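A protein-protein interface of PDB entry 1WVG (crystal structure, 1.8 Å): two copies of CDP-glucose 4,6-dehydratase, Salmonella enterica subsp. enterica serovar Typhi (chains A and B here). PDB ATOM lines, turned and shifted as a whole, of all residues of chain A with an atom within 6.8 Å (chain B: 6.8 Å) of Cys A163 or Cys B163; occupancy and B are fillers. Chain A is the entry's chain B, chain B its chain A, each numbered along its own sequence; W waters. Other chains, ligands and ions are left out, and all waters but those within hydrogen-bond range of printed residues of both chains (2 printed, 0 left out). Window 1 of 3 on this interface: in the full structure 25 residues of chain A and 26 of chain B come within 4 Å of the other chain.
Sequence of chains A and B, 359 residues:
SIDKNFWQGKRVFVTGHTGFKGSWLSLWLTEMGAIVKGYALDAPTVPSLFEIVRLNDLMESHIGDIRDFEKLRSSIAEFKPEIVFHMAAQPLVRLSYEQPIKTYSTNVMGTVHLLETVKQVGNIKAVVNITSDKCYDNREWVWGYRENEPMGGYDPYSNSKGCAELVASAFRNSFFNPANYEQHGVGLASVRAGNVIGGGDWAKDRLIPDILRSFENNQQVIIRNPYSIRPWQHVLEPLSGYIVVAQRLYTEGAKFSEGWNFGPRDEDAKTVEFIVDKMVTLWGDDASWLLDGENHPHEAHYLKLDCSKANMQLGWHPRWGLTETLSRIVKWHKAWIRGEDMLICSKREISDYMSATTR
Gly A152 touches Leu B166, but with the chains exchanged Leu A166 does not touch Gly B152 (4.04 Å).
Asn A159 touches Leu B166, and with the chains exchanged Leu A166 touches Asn B159.
Asn A159 touches Val B167, and with the chains exchanged Val A167 touches Asn B159.
Cys A163 touches its own counterpart, Cys B163.
18 positions are printed for both chains.
Of the 12 pairs that touch across the chains among the printed residues, 11 have their exchanged pair printed and touching as well.
The side-chain amide oxygen (OD1) of Asn A159 is in hydrogen-bond range of the backbone NH (N) of Val B167 (3.4 Å).
The backbone carbonyl oxygen (O) of Leu A166 is in hydrogen-bond range of the side-chain amide nitrogen (ND2) of Asn B159, at 2.8 Å.
The side-chain amide nitrogen (ND2) of Asn A159 lies within hydrogen-bond range of the backbone carbonyl oxygen (O) of Leu B166.
The backbone carbonyl oxygen (O) of Cys A163 sits at hydrogen-bond distance from the side-chain sulfur (SG) of Cys B163 (3.7 Å).
O of Asn A159 sits at hydrogen-bond distance from SG of Cys A163 (3.5 Å).
The side-chain amide oxygen (OD1) of Asn B159 is in hydrogen-bond range of the side-chain hydroxyl (OH) of Tyr B104 (2.7 Å).
The side-chain sulfur of Cys B163 sits at hydrogen-bond distance from the backbone carbonyl oxygen of Asn B159, 3.5 Å away.
The side-chain hydroxyl (OH) of Tyr A104 is in hydrogen-bond range of the side-chain amide oxygen (OD1) of Asn A159.
The backbone carbonyl oxygen (O) of Cys A135 sits at hydrogen-bond distance from the backbone NH (N) of Gly A152 (2.8 Å).
Of chain B, only Cys B163 and Leu B166 come within 4 Å of Cys A163.
Cys B163 touches just these residues of chain A: Cys A163 and Leu A166.
Gly A162 touches just one residue of chain B: Leu B166.
Gly B162 touches just one residue of chain A: Leu A166 (3.6 Å).
Printed residues of chain B within 4 Å of Leu A166: Asn B159 (2.8 Å), Gly B162 (3.6 Å) and Cys B163 (3.7 Å).
Of the printed residues of chain A, Tyr B104 touches Val A167.
Of the printed residues of chain A, Asn B159 touches Leu A166 (2.8 Å) and Val A167 (3.5 Å).
Of the printed residues of chain A, Val B167 touches Tyr A104 (3.9 Å) and Asn A159 (3.4 Å).
The nearest residue of chain B that does not touch Cys A163 is Val B167 (4.3 Å).
The nearest printed residue of chain B that does not touch Leu A166 is Gly B152 (4.04 Å).
Among the printed residues, merely in contact across the chains: Tyr A104 with Val B167, Gly A152 with Leu B166, Gly A162 with Leu B166, Cys A163 with Leu B166, Leu A166 with Gly B162, Leu A166 with Cys B163, Val A167 with Tyr B104 and Val A167 with Asn B159.
Water W2 lies within hydrogen-bond range of the backbone NH of Met A151 and the backbone carbonyl oxygen of Met B151.
Water W1 lies within hydrogen-bond range of N of Met B151 (2.9 Å) and O of Met A151 (3.0 Å).
Of the 19 printed residues of chain A, 7 touch a printed residue of chain B.
Printed residues of chain A that touch a printed residue of chain B: Tyr A104, Gly A152, Asn A159, Gly A162, Cys A163, Leu A166 and Val A167.
Hydrophobic or aromatic side chains of chain A within 4 Å of the printed part of chain B: Tyr A104, Leu A166 and Val A167.
Of the 18 printed residues of chain B, 6 touch a printed residue of chain A.
Hydrophobic or aromatic side chains of chain B within 4 Å of the printed part of chain A: Tyr B104, Leu B166 and Val B167.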
ATOM      1  N   TYR A 104      22.829  23.113  13.516  1.00  0.00           N
ATOM      2  CA  TYR A 104      21.889  23.063  12.428  1.00  0.00           C
ATOM      3  C   TYR A 104      21.849  24.322  11.595  1.00  0.00           C
ATOM      4  O   TYR A 104      21.836  24.307  10.355  1.00  0.00           O
ATOM      5  CB  TYR A 104      20.481  22.651  12.924  1.00  0.00           C
ATOM      6  CG  TYR A 104      20.270  21.140  13.187  1.00  0.00           C
ATOM      7  CD1 TYR A 104      20.194  20.634  14.486  1.00  0.00           C
ATOM      8  CD2 TYR A 104      20.078  20.224  12.143  1.00  0.00           C
ATOM      9  CE1 TYR A 104      19.965  19.282  14.750  1.00  0.00           C
ATOM     10  CE2 TYR A 104      19.856  18.865  12.375  1.00  0.00           C
ATOM     11  CZ  TYR A 104      19.811  18.386  13.687  1.00  0.00           C
ATOM     12  OH  TYR A 104      19.546  17.045  13.930  1.00  0.00           O
ATOM     13  N   ASN A 107      25.241  24.327   9.732  1.00  0.00           N
ATOM     14  CA  ASN A 107      25.315  23.224   8.782  1.00  0.00           C
ATOM     15  C   ASN A 107      24.184  23.134   7.730  1.00  0.00           C
ATOM     16  O   ASN A 107      24.397  22.847   6.547  1.00  0.00           O
ATOM     17  CB  ASN A 107      25.605  21.884   9.512  1.00  0.00           C
ATOM     18  CG  ASN A 107      26.957  21.853  10.232  1.00  0.00           C
ATOM     19  OD1 ASN A 107      27.875  22.629   9.951  1.00  0.00           O
ATOM     20  ND2 ASN A 107      27.113  20.923  11.150  1.00  0.00           N
ATOM     21  N   VAL A 108      22.942  23.386   8.119  1.00  0.00           N
ATOM     22  CA  VAL A 108      21.874  23.283   7.141  1.00  0.00           C
ATOM     23  C   VAL A 108      21.557  24.647   6.495  1.00  0.00           C
ATOM     24  O   VAL A 108      21.604  24.817   5.260  1.00  0.00           O
ATOM     25  CB  VAL A 108      20.667  22.567   7.752  1.00  0.00           C
ATOM     26  CG1 VAL A 108      19.452  22.534   6.796  1.00  0.00           C
ATOM     27  CG2 VAL A 108      21.076  21.156   8.240  1.00  0.00           C
ATOM     28  N   THR A 111      24.190  25.900   4.164  1.00  0.00           N
ATOM     29  CA  THR A 111      24.189  25.177   2.885  1.00  0.00           C
ATOM     30  C   THR A 111      23.111  25.725   1.961  1.00  0.00           C
ATOM     31  O   THR A 111      23.284  25.954   0.761  1.00  0.00           O
ATOM     32  CB  THR A 111      24.017  23.648   3.137  1.00  0.00           C
ATOM     33  OG1 THR A 111      25.167  23.176   3.824  1.00  0.00           O
ATOM     34  CG2 THR A 111      23.777  22.808   1.858  1.00  0.00           C
ATOM     35  N   CYS A 135      26.845  11.477   7.129  1.00  0.00           N
ATOM     36  CA  CYS A 135      25.567  11.870   6.668  1.00  0.00           C
ATOM     37  C   CYS A 135      24.631  10.670   6.565  1.00  0.00           C
ATOM     38  O   CYS A 135      23.397  10.776   6.632  1.00  0.00           O
ATOM     39  CB  CYS A 135      25.773  12.540   5.303  1.00  0.00           C
ATOM     40  SG  CYS A 135      26.389  11.440   3.989  1.00  0.00           S
ATOM     41  N   MET A 151      19.934   8.847   4.001  1.00  0.00           N
ATOM     42  CA  MET A 151      20.622   9.785   4.904  1.00  0.00           C
ATOM     43  C   MET A 151      19.990   9.782   6.266  1.00  0.00           C
ATOM     44  O   MET A 151      18.845   9.347   6.402  1.00  0.00           O
ATOM     45  CB  MET A 151      20.546  11.206   4.333  1.00  0.00           C
ATOM     46  CG  MET A 151      21.212  11.299   2.949  1.00  0.00           C
ATOM     47  SD  MET A 151      23.009  11.082   3.084  1.00  0.00           S
ATOM     48  CE  MET A 151      23.621  10.333   1.548  1.00  0.00           C
ATOM     49  N   GLY A 152      20.729  10.251   7.267  1.00  0.00           N
ATOM     50  CA  GLY A 152      20.249  10.307   8.639  1.00  0.00           C
ATOM     51  C   GLY A 152      21.303  10.901   9.536  1.00  0.00           C
ATOM     52  O   GLY A 152      21.900  11.914   9.264  1.00  0.00           O
ATOM     53  N   SER A 158      25.977  14.787  12.941  1.00  0.00           N
ATOM     54  CA  SER A 158      25.784  13.785  11.902  1.00  0.00           C
ATOM     55  C   SER A 158      24.500  14.022  11.198  1.00  0.00           C
ATOM     56  O   SER A 158      24.457  14.008   9.968  1.00  0.00           O
ATOM     57  CB  SER A 158      25.704  12.432  12.541  1.00  0.00           C
ATOM     58  OG  SER A 158      26.989  12.123  13.054  1.00  0.00           O
ATOM     59  N   ASN A 159      23.459  14.250  12.016  1.00  0.00           N
ATOM     60  CA  ASN A 159      22.134  14.527  11.476  1.00  0.00           C
ATOM     61  C   ASN A 159      22.129  15.795  10.616  1.00  0.00           C
ATOM     62  O   ASN A 159      21.475  15.851   9.551  1.00  0.00           O
ATOM     63  CB  ASN A 159      21.064  14.533  12.580  1.00  0.00           C
ATOM     64  CG  ASN A 159      19.623  14.456  12.097  1.00  0.00           C
ATOM     65  OD1 ASN A 159      18.926  15.451  11.986  1.00  0.00           O
ATOM     66  ND2 ASN A 159      19.129  13.254  11.874  1.00  0.00           N
ATOM     67  N   SER A 160      22.876  16.827  11.056  1.00  0.00           N
ATOM     68  CA  SER A 160      22.949  18.085  10.322  1.00  0.00           C
ATOM     69  C   SER A 160      23.494  17.889   8.906  1.00  0.00           C
ATOM     70  O   SER A 160      23.094  18.535   7.929  1.00  0.00           O
ATOM     71  CB  SER A 160      23.689  19.172  11.093  1.00  0.00           C
ATOM     72  OG  SER A 160      25.080  18.972  11.060  1.00  0.00           O
ATOM     73  N   LYS A 161      24.428  16.951   8.820  1.00  0.00           N
ATOM     74  CA  LYS A 161      25.071  16.556   7.567  1.00  0.00           C
ATOM     75  C   LYS A 161      24.110  15.733   6.681  1.00  0.00           C
ATOM     76  O   LYS A 161      24.129  15.803   5.448  1.00  0.00           O
ATOM     77  CB  LYS A 161      26.387  15.835   7.835  1.00  0.00           C
ATOM     78  CG  LYS A 161      27.354  16.804   8.493  1.00  0.00           C
ATOM     79  CD  LYS A 161      27.867  17.862   7.529  1.00  0.00           C
ATOM     80  CE  LYS A 161      29.233  18.385   7.949  1.00  0.00           C
ATOM     81  NZ  LYS A 161      29.952  19.085   6.861  1.00  0.00           N
ATOM     82  N   GLY A 162      23.239  14.948   7.304  1.00  0.00           N
ATOM     83  CA  GLY A 162      22.299  14.204   6.490  1.00  0.00           C
ATOM     84  C   GLY A 162      21.331  15.219   5.886  1.00  0.00           C
ATOM     85  O   GLY A 162      20.882  15.085   4.753  1.00  0.00           O
ATOM     86  N   CYS A 163      20.999  16.272   6.654  1.00  0.00           N
ATOM     87  CA  CYS A 163      20.098  17.304   6.154  1.00  0.00           C
ATOM     88  C   CYS A 163      20.729  18.116   5.002  1.00  0.00           C
ATOM     89  O   CYS A 163      20.106  18.451   3.961  1.00  0.00           O
ATOM     90  CB  CYS A 163      19.677  18.269   7.290  1.00  0.00           C
ATOM     91  SG  CYS A 163      18.556  17.527   8.505  1.00  0.00           S
ATOM     92  N   ALA A 164      22.008  18.417   5.184  1.00  0.00           N
ATOM     93  CA  ALA A 164      22.735  19.182   4.167  1.00  0.00           C
ATOM     94  C   ALA A 164      22.741  18.427   2.868  1.00  0.00           C
ATOM     95  O   ALA A 164      22.675  18.984   1.766  1.00  0.00           O
ATOM     96  CB  ALA A 164      24.163  19.411   4.635  1.00  0.00           C
ATOM     97  N   GLU A 165      22.823  17.113   3.029  1.00  0.00           N
ATOM     98  CA  GLU A 165      22.797  16.247   1.885  1.00  0.00           C
ATOM     99  C   GLU A 165      21.411  16.306   1.239  1.00  0.00           C
ATOM    100  O   GLU A 165      21.314  16.321   0.010  1.00  0.00           O
ATOM    101  CB  GLU A 165      23.165  14.803   2.246  1.00  0.00           C
ATOM    102  CG  GLU A 165      24.691  14.601   2.347  1.00  0.00           C
ATOM    103  CD  GLU A 165      25.343  14.520   1.007  1.00  0.00           C
ATOM    104  OE1 GLU A 165      24.726  14.500  -0.045  1.00  0.00           O
ATOM    105  OE2 GLU A 165      26.627  14.415   1.096  1.00  0.00           O
ATOM    106  N   LEU A 166      20.342  16.358   2.058  1.00  0.00           N
ATOM    107  CA  LEU A 166      18.998  16.444   1.478  1.00  0.00           C
ATOM    108  C   LEU A 166      18.875  17.785   0.770  1.00  0.00           C
ATOM    109  O   LEU A 166      18.316  17.898  -0.329  1.00  0.00           O
ATOM    110  CB  LEU A 166      17.833  16.310   2.513  1.00  0.00           C
ATOM    111  CG  LEU A 166      17.254  14.896   2.648  1.00  0.00           C
ATOM    112  CD1 LEU A 166      18.330  13.988   3.219  1.00  0.00           C
ATOM    113  CD2 LEU A 166      16.086  14.836   3.618  1.00  0.00           C
ATOM    114  N   VAL A 167      19.388  18.822   1.442  1.00  0.00           N
ATOM    115  CA  VAL A 167      19.341  20.153   0.819  1.00  0.00           C
ATOM    116  C   VAL A 167      19.987  20.177  -0.583  1.00  0.00           C
ATOM    117  O   VAL A 167      19.412  20.656  -1.571  1.00  0.00           O
ATOM    118  CB  VAL A 167      20.096  21.172   1.685  1.00  0.00           C
ATOM    119  CG1 VAL A 167      20.137  22.504   0.933  1.00  0.00           C
ATOM    120  CG2 VAL A 167      19.385  21.364   3.017  1.00  0.00           C
ATOM    121  N   ALA A 168      21.238  19.725  -0.673  1.00  0.00           N
ATOM    122  CA  ALA A 168      21.928  19.737  -1.955  1.00  0.00           C
ATOM    123  C   ALA A 168      21.152  19.021  -3.034  1.00  0.00           C
ATOM    124  O   ALA A 168      21.162  19.424  -4.195  1.00  0.00           O
ATOM    125  CB  ALA A 168      23.295  19.117  -1.860  1.00  0.00           C
ATOM    126  N   SER A 169      20.487  17.926  -2.650  1.00  0.00           N
ATOM    127  CA  SER A 169      19.699  17.132  -3.581  1.00  0.00           C
ATOM    128  C   SER A 169      18.524  17.879  -4.129  1.00  0.00           C
ATOM    129  O   SER A 169      18.262  17.810  -5.319  1.00  0.00           O
ATOM    130  CB  SER A 169      19.168  15.879  -2.888  1.00  0.00           C
ATOM    131  OG  SER A 169      20.279  15.039  -2.675  1.00  0.00           O
ATOM    132  N   TYR B 104      12.978  26.507   4.217  1.00  0.00           N
ATOM    133  CA  TYR B 104      13.868  25.745   5.047  1.00  0.00           C
ATOM    134  C   TYR B 104      14.016  26.290   6.458  1.00  0.00           C
ATOM    135  O   TYR B 104      14.004  25.541   7.464  1.00  0.00           O
ATOM    136  CB  TYR B 104      15.235  25.652   4.370  1.00  0.00           C
ATOM    137  CG  TYR B 104      15.328  24.545   3.341  1.00  0.00           C
ATOM    138  CD1 TYR B 104      15.300  24.857   1.978  1.00  0.00           C
ATOM    139  CD2 TYR B 104      15.484  23.200   3.715  1.00  0.00           C
ATOM    140  CE1 TYR B 104      15.422  23.853   1.014  1.00  0.00           C
ATOM    141  CE2 TYR B 104      15.622  22.184   2.763  1.00  0.00           C
ATOM    142  CZ  TYR B 104      15.585  22.520   1.407  1.00  0.00           C
ATOM    143  OH  TYR B 104      15.719  21.548   0.441  1.00  0.00           O
ATOM    144  N   ASN B 107      10.590  25.565   8.251  1.00  0.00           N
ATOM    145  CA  ASN B 107      10.340  24.157   8.485  1.00  0.00           C
ATOM    146  C   ASN B 107      11.422  23.436   9.245  1.00  0.00           C
ATOM    147  O   ASN B 107      11.165  22.655  10.165  1.00  0.00           O
ATOM    148  CB  ASN B 107       9.963  23.466   7.160  1.00  0.00           C
ATOM    149  CG  ASN B 107       8.718  24.128   6.572  1.00  0.00           C
ATOM    150  OD1 ASN B 107       8.024  24.929   7.234  1.00  0.00           O
ATOM    151  ND2 ASN B 107       8.389  23.770   5.332  1.00  0.00           N
ATOM    152  N   VAL B 108      12.645  23.697   8.852  1.00  0.00           N
ATOM    153  CA  VAL B 108      13.742  23.039   9.523  1.00  0.00           C
ATOM    154  C   VAL B 108      14.127  23.638  10.896  1.00  0.00           C
ATOM    155  O   VAL B 108      13.990  22.977  11.934  1.00  0.00           O
ATOM    156  CB  VAL B 108      14.909  22.908   8.560  1.00  0.00           C
ATOM    157  CG1 VAL B 108      15.977  22.061   9.215  1.00  0.00           C
ATOM    158  CG2 VAL B 108      14.428  22.297   7.234  1.00  0.00           C
ATOM    159  N   THR B 111      11.582  23.604  13.528  1.00  0.00           N
ATOM    160  CA  THR B 111      11.460  22.318  14.243  1.00  0.00           C
ATOM    161  C   THR B 111      12.540  22.188  15.299  1.00  0.00           C
ATOM    162  O   THR B 111      12.305  21.771  16.433  1.00  0.00           O
ATOM    163  CB  THR B 111      11.562  21.168  13.239  1.00  0.00           C
ATOM    164  OG1 THR B 111      10.450  21.328  12.381  1.00  0.00           O
ATOM    165  CG2 THR B 111      11.461  19.823  13.965  1.00  0.00           C
ATOM    166  N   CYS B 135       7.616  13.860   2.922  1.00  0.00           N
ATOM    167  CA  CYS B 135       8.956  13.624   3.488  1.00  0.00           C
ATOM    168  C   CYS B 135       9.743  12.490   2.826  1.00  0.00           C
ATOM    169  O   CYS B 135      11.001  12.450   2.824  1.00  0.00           O
ATOM    170  CB  CYS B 135       8.919  13.423   5.031  1.00  0.00           C
ATOM    171  SG  CYS B 135       8.082  11.884   5.541  1.00  0.00           S
ATOM    172  N   MET B 151      13.912   9.203   3.559  1.00  0.00           N
ATOM    173  CA  MET B 151      13.464  10.578   3.555  1.00  0.00           C
ATOM    174  C   MET B 151      14.121  11.252   2.367  1.00  0.00           C
ATOM    175  O   MET B 151      15.197  10.851   1.925  1.00  0.00           O
ATOM    176  CB  MET B 151      13.891  11.326   4.843  1.00  0.00           C
ATOM    177  CG  MET B 151      13.253  10.794   6.111  1.00  0.00           C
ATOM    178  SD  MET B 151      11.468  10.807   5.975  1.00  0.00           S
ATOM    179  CE  MET B 151      10.990   9.112   6.396  1.00  0.00           C
ATOM    180  N   GLY B 152      13.461  12.267   1.831  1.00  0.00           N
ATOM    181  CA  GLY B 152      14.005  12.993   0.688  1.00  0.00           C
ATOM    182  C   GLY B 152      13.138  14.203   0.418  1.00  0.00           C
ATOM    183  O   GLY B 152      12.710  14.907   1.357  1.00  0.00           O
ATOM    184  N   SER B 158       8.960  19.707   0.106  1.00  0.00           N
ATOM    185  CA  SER B 158       9.067  18.276   0.357  1.00  0.00           C
ATOM    186  C   SER B 158      10.309  17.959   1.132  1.00  0.00           C
ATOM    187  O   SER B 158      10.263  17.302   2.167  1.00  0.00           O
ATOM    188  CB  SER B 158       9.220  17.545  -0.943  1.00  0.00           C
ATOM    189  OG  SER B 158       8.003  17.746  -1.614  1.00  0.00           O
ATOM    190  N   ASN B 159      11.422  18.417   0.564  1.00  0.00           N
ATOM    191  CA  ASN B 159      12.747  18.216   1.125  1.00  0.00           C
ATOM    192  C   ASN B 159      12.914  18.805   2.536  1.00  0.00           C
ATOM    193  O   ASN B 159      13.606  18.230   3.375  1.00  0.00           O
ATOM    194  CB  ASN B 159      13.808  18.734   0.128  1.00  0.00           C
ATOM    195  CG  ASN B 159      15.201  18.318   0.521  1.00  0.00           C
ATOM    196  OD1 ASN B 159      15.874  19.007   1.283  1.00  0.00           O
ATOM    197  ND2 ASN B 159      15.639  17.161   0.026  1.00  0.00           N
ATOM    198  N   SER B 160      12.255  19.944   2.822  1.00  0.00           N
ATOM    199  CA  SER B 160      12.359  20.537   4.152  1.00  0.00           C
ATOM    200  C   SER B 160      11.720  19.629   5.228  1.00  0.00           C
ATOM    201  O   SER B 160      12.121  19.616   6.392  1.00  0.00           O
ATOM    202  CB  SER B 160      11.827  21.971   4.150  1.00  0.00           C
ATOM    203  OG  SER B 160      10.419  21.939   3.950  1.00  0.00           O
ATOM    204  N   LYS B 161      10.687  18.867   4.820  1.00  0.00           N
ATOM    205  CA  LYS B 161       9.924  17.910   5.682  1.00  0.00           C
ATOM    206  C   LYS B 161      10.734  16.630   5.970  1.00  0.00           C
ATOM    207  O   LYS B 161      10.713  16.001   7.059  1.00  0.00           O
ATOM    208  CB  LYS B 161       8.573  17.613   5.043  1.00  0.00           C
ATOM    209  CG  LYS B 161       7.699  18.843   5.092  1.00  0.00           C
ATOM    210  CD  LYS B 161       7.384  19.213   6.532  1.00  0.00           C
ATOM    211  CE  LYS B 161       6.477  20.413   6.602  1.00  0.00           C
ATOM    212  NZ  LYS B 161       5.610  20.365   7.778  1.00  0.00           N
ATOM    213  N   GLY B 162      11.487  16.271   4.930  1.00  0.00           N
ATOM    214  CA  GLY B 162      12.436  15.181   4.941  1.00  0.00           C
ATOM    215  C   GLY B 162      13.448  15.544   6.016  1.00  0.00           C
ATOM    216  O   GLY B 162      13.699  14.773   6.925  1.00  0.00           O
ATOM    217  N   CYS B 163      13.988  16.766   5.935  1.00  0.00           N
ATOM    218  CA  CYS B 163      14.922  17.249   6.942  1.00  0.00           C
ATOM    219  C   CYS B 163      14.245  17.349   8.309  1.00  0.00           C
ATOM    220  O   CYS B 163      14.879  17.028   9.323  1.00  0.00           O
ATOM    221  CB  CYS B 163      15.467  18.635   6.600  1.00  0.00           C
ATOM    222  SG  CYS B 163      16.563  18.634   5.159  1.00  0.00           S
ATOM    223  N   ALA B 164      12.983  17.825   8.357  1.00  0.00           N
ATOM    224  CA  ALA B 164      12.266  17.927   9.651  1.00  0.00           C
ATOM    225  C   ALA B 164      12.166  16.534  10.301  1.00  0.00           C
ATOM    226  O   ALA B 164      12.270  16.346  11.516  1.00  0.00           O
ATOM    227  CB  ALA B 164      10.900  18.615   9.518  1.00  0.00           C
ATOM    228  N   GLU B 165      11.988  15.506   9.459  1.00  0.00           N
ATOM    229  CA  GLU B 165      11.917  14.131   9.955  1.00  0.00           C
ATOM    230  C   GLU B 165      13.242  13.724  10.564  1.00  0.00           C
ATOM    231  O   GLU B 165      13.311  13.163  11.654  1.00  0.00           O
ATOM    232  CB  GLU B 165      11.604  13.204   8.759  1.00  0.00           C
ATOM    233  CG  GLU B 165      10.091  13.072   8.558  1.00  0.00           C
ATOM    234  CD  GLU B 165       9.418  12.277   9.654  1.00  0.00           C
ATOM    235  OE1 GLU B 165      10.013  11.517  10.379  1.00  0.00           O
ATOM    236  OE2 GLU B 165       8.129  12.459   9.732  1.00  0.00           O
ATOM    237  N   LEU B 166      14.333  14.040   9.872  1.00  0.00           N
ATOM    238  CA  LEU B 166      15.674  13.713  10.362  1.00  0.00           C
ATOM    239  C   LEU B 166      15.947  14.416  11.686  1.00  0.00           C
ATOM    240  O   LEU B 166      16.490  13.857  12.644  1.00  0.00           O
ATOM    241  CB  LEU B 166      16.774  14.157   9.348  1.00  0.00           C
ATOM    242  CG  LEU B 166      17.310  13.072   8.396  1.00  0.00           C
ATOM    243  CD1 LEU B 166      16.220  12.531   7.473  1.00  0.00           C
ATOM    244  CD2 LEU B 166      18.442  13.650   7.567  1.00  0.00           C
ATOM    245  N   VAL B 167      15.572  15.684  11.725  1.00  0.00           N
ATOM    246  CA  VAL B 167      15.777  16.477  12.923  1.00  0.00           C
ATOM    247  C   VAL B 167      15.140  15.857  14.149  1.00  0.00           C
ATOM    248  O   VAL B 167      15.791  15.735  15.188  1.00  0.00           O
ATOM    249  CB  VAL B 167      15.190  17.848  12.745  1.00  0.00           C
ATOM    250  CG1 VAL B 167      15.050  18.487  14.131  1.00  0.00           C
ATOM    251  CG2 VAL B 167      16.044  18.666  11.784  1.00  0.00           C
ATOM    252  N   ALA B 168      13.853  15.507  14.036  1.00  0.00           N
ATOM    253  CA  ALA B 168      13.129  14.896  15.158  1.00  0.00           C
ATOM    254  C   ALA B 168      13.755  13.557  15.577  1.00  0.00           C
ATOM    255  O   ALA B 168      13.873  13.205  16.756  1.00  0.00           O
ATOM    256  CB  ALA B 168      11.675  14.663  14.774  1.00  0.00           C
HETATM  257  O   HOH W   1      16.128   8.536   5.343  1.00  0.00           O
HETATM  258  O   HOH W   2      17.729   9.462   2.484  1.00  0.00           O
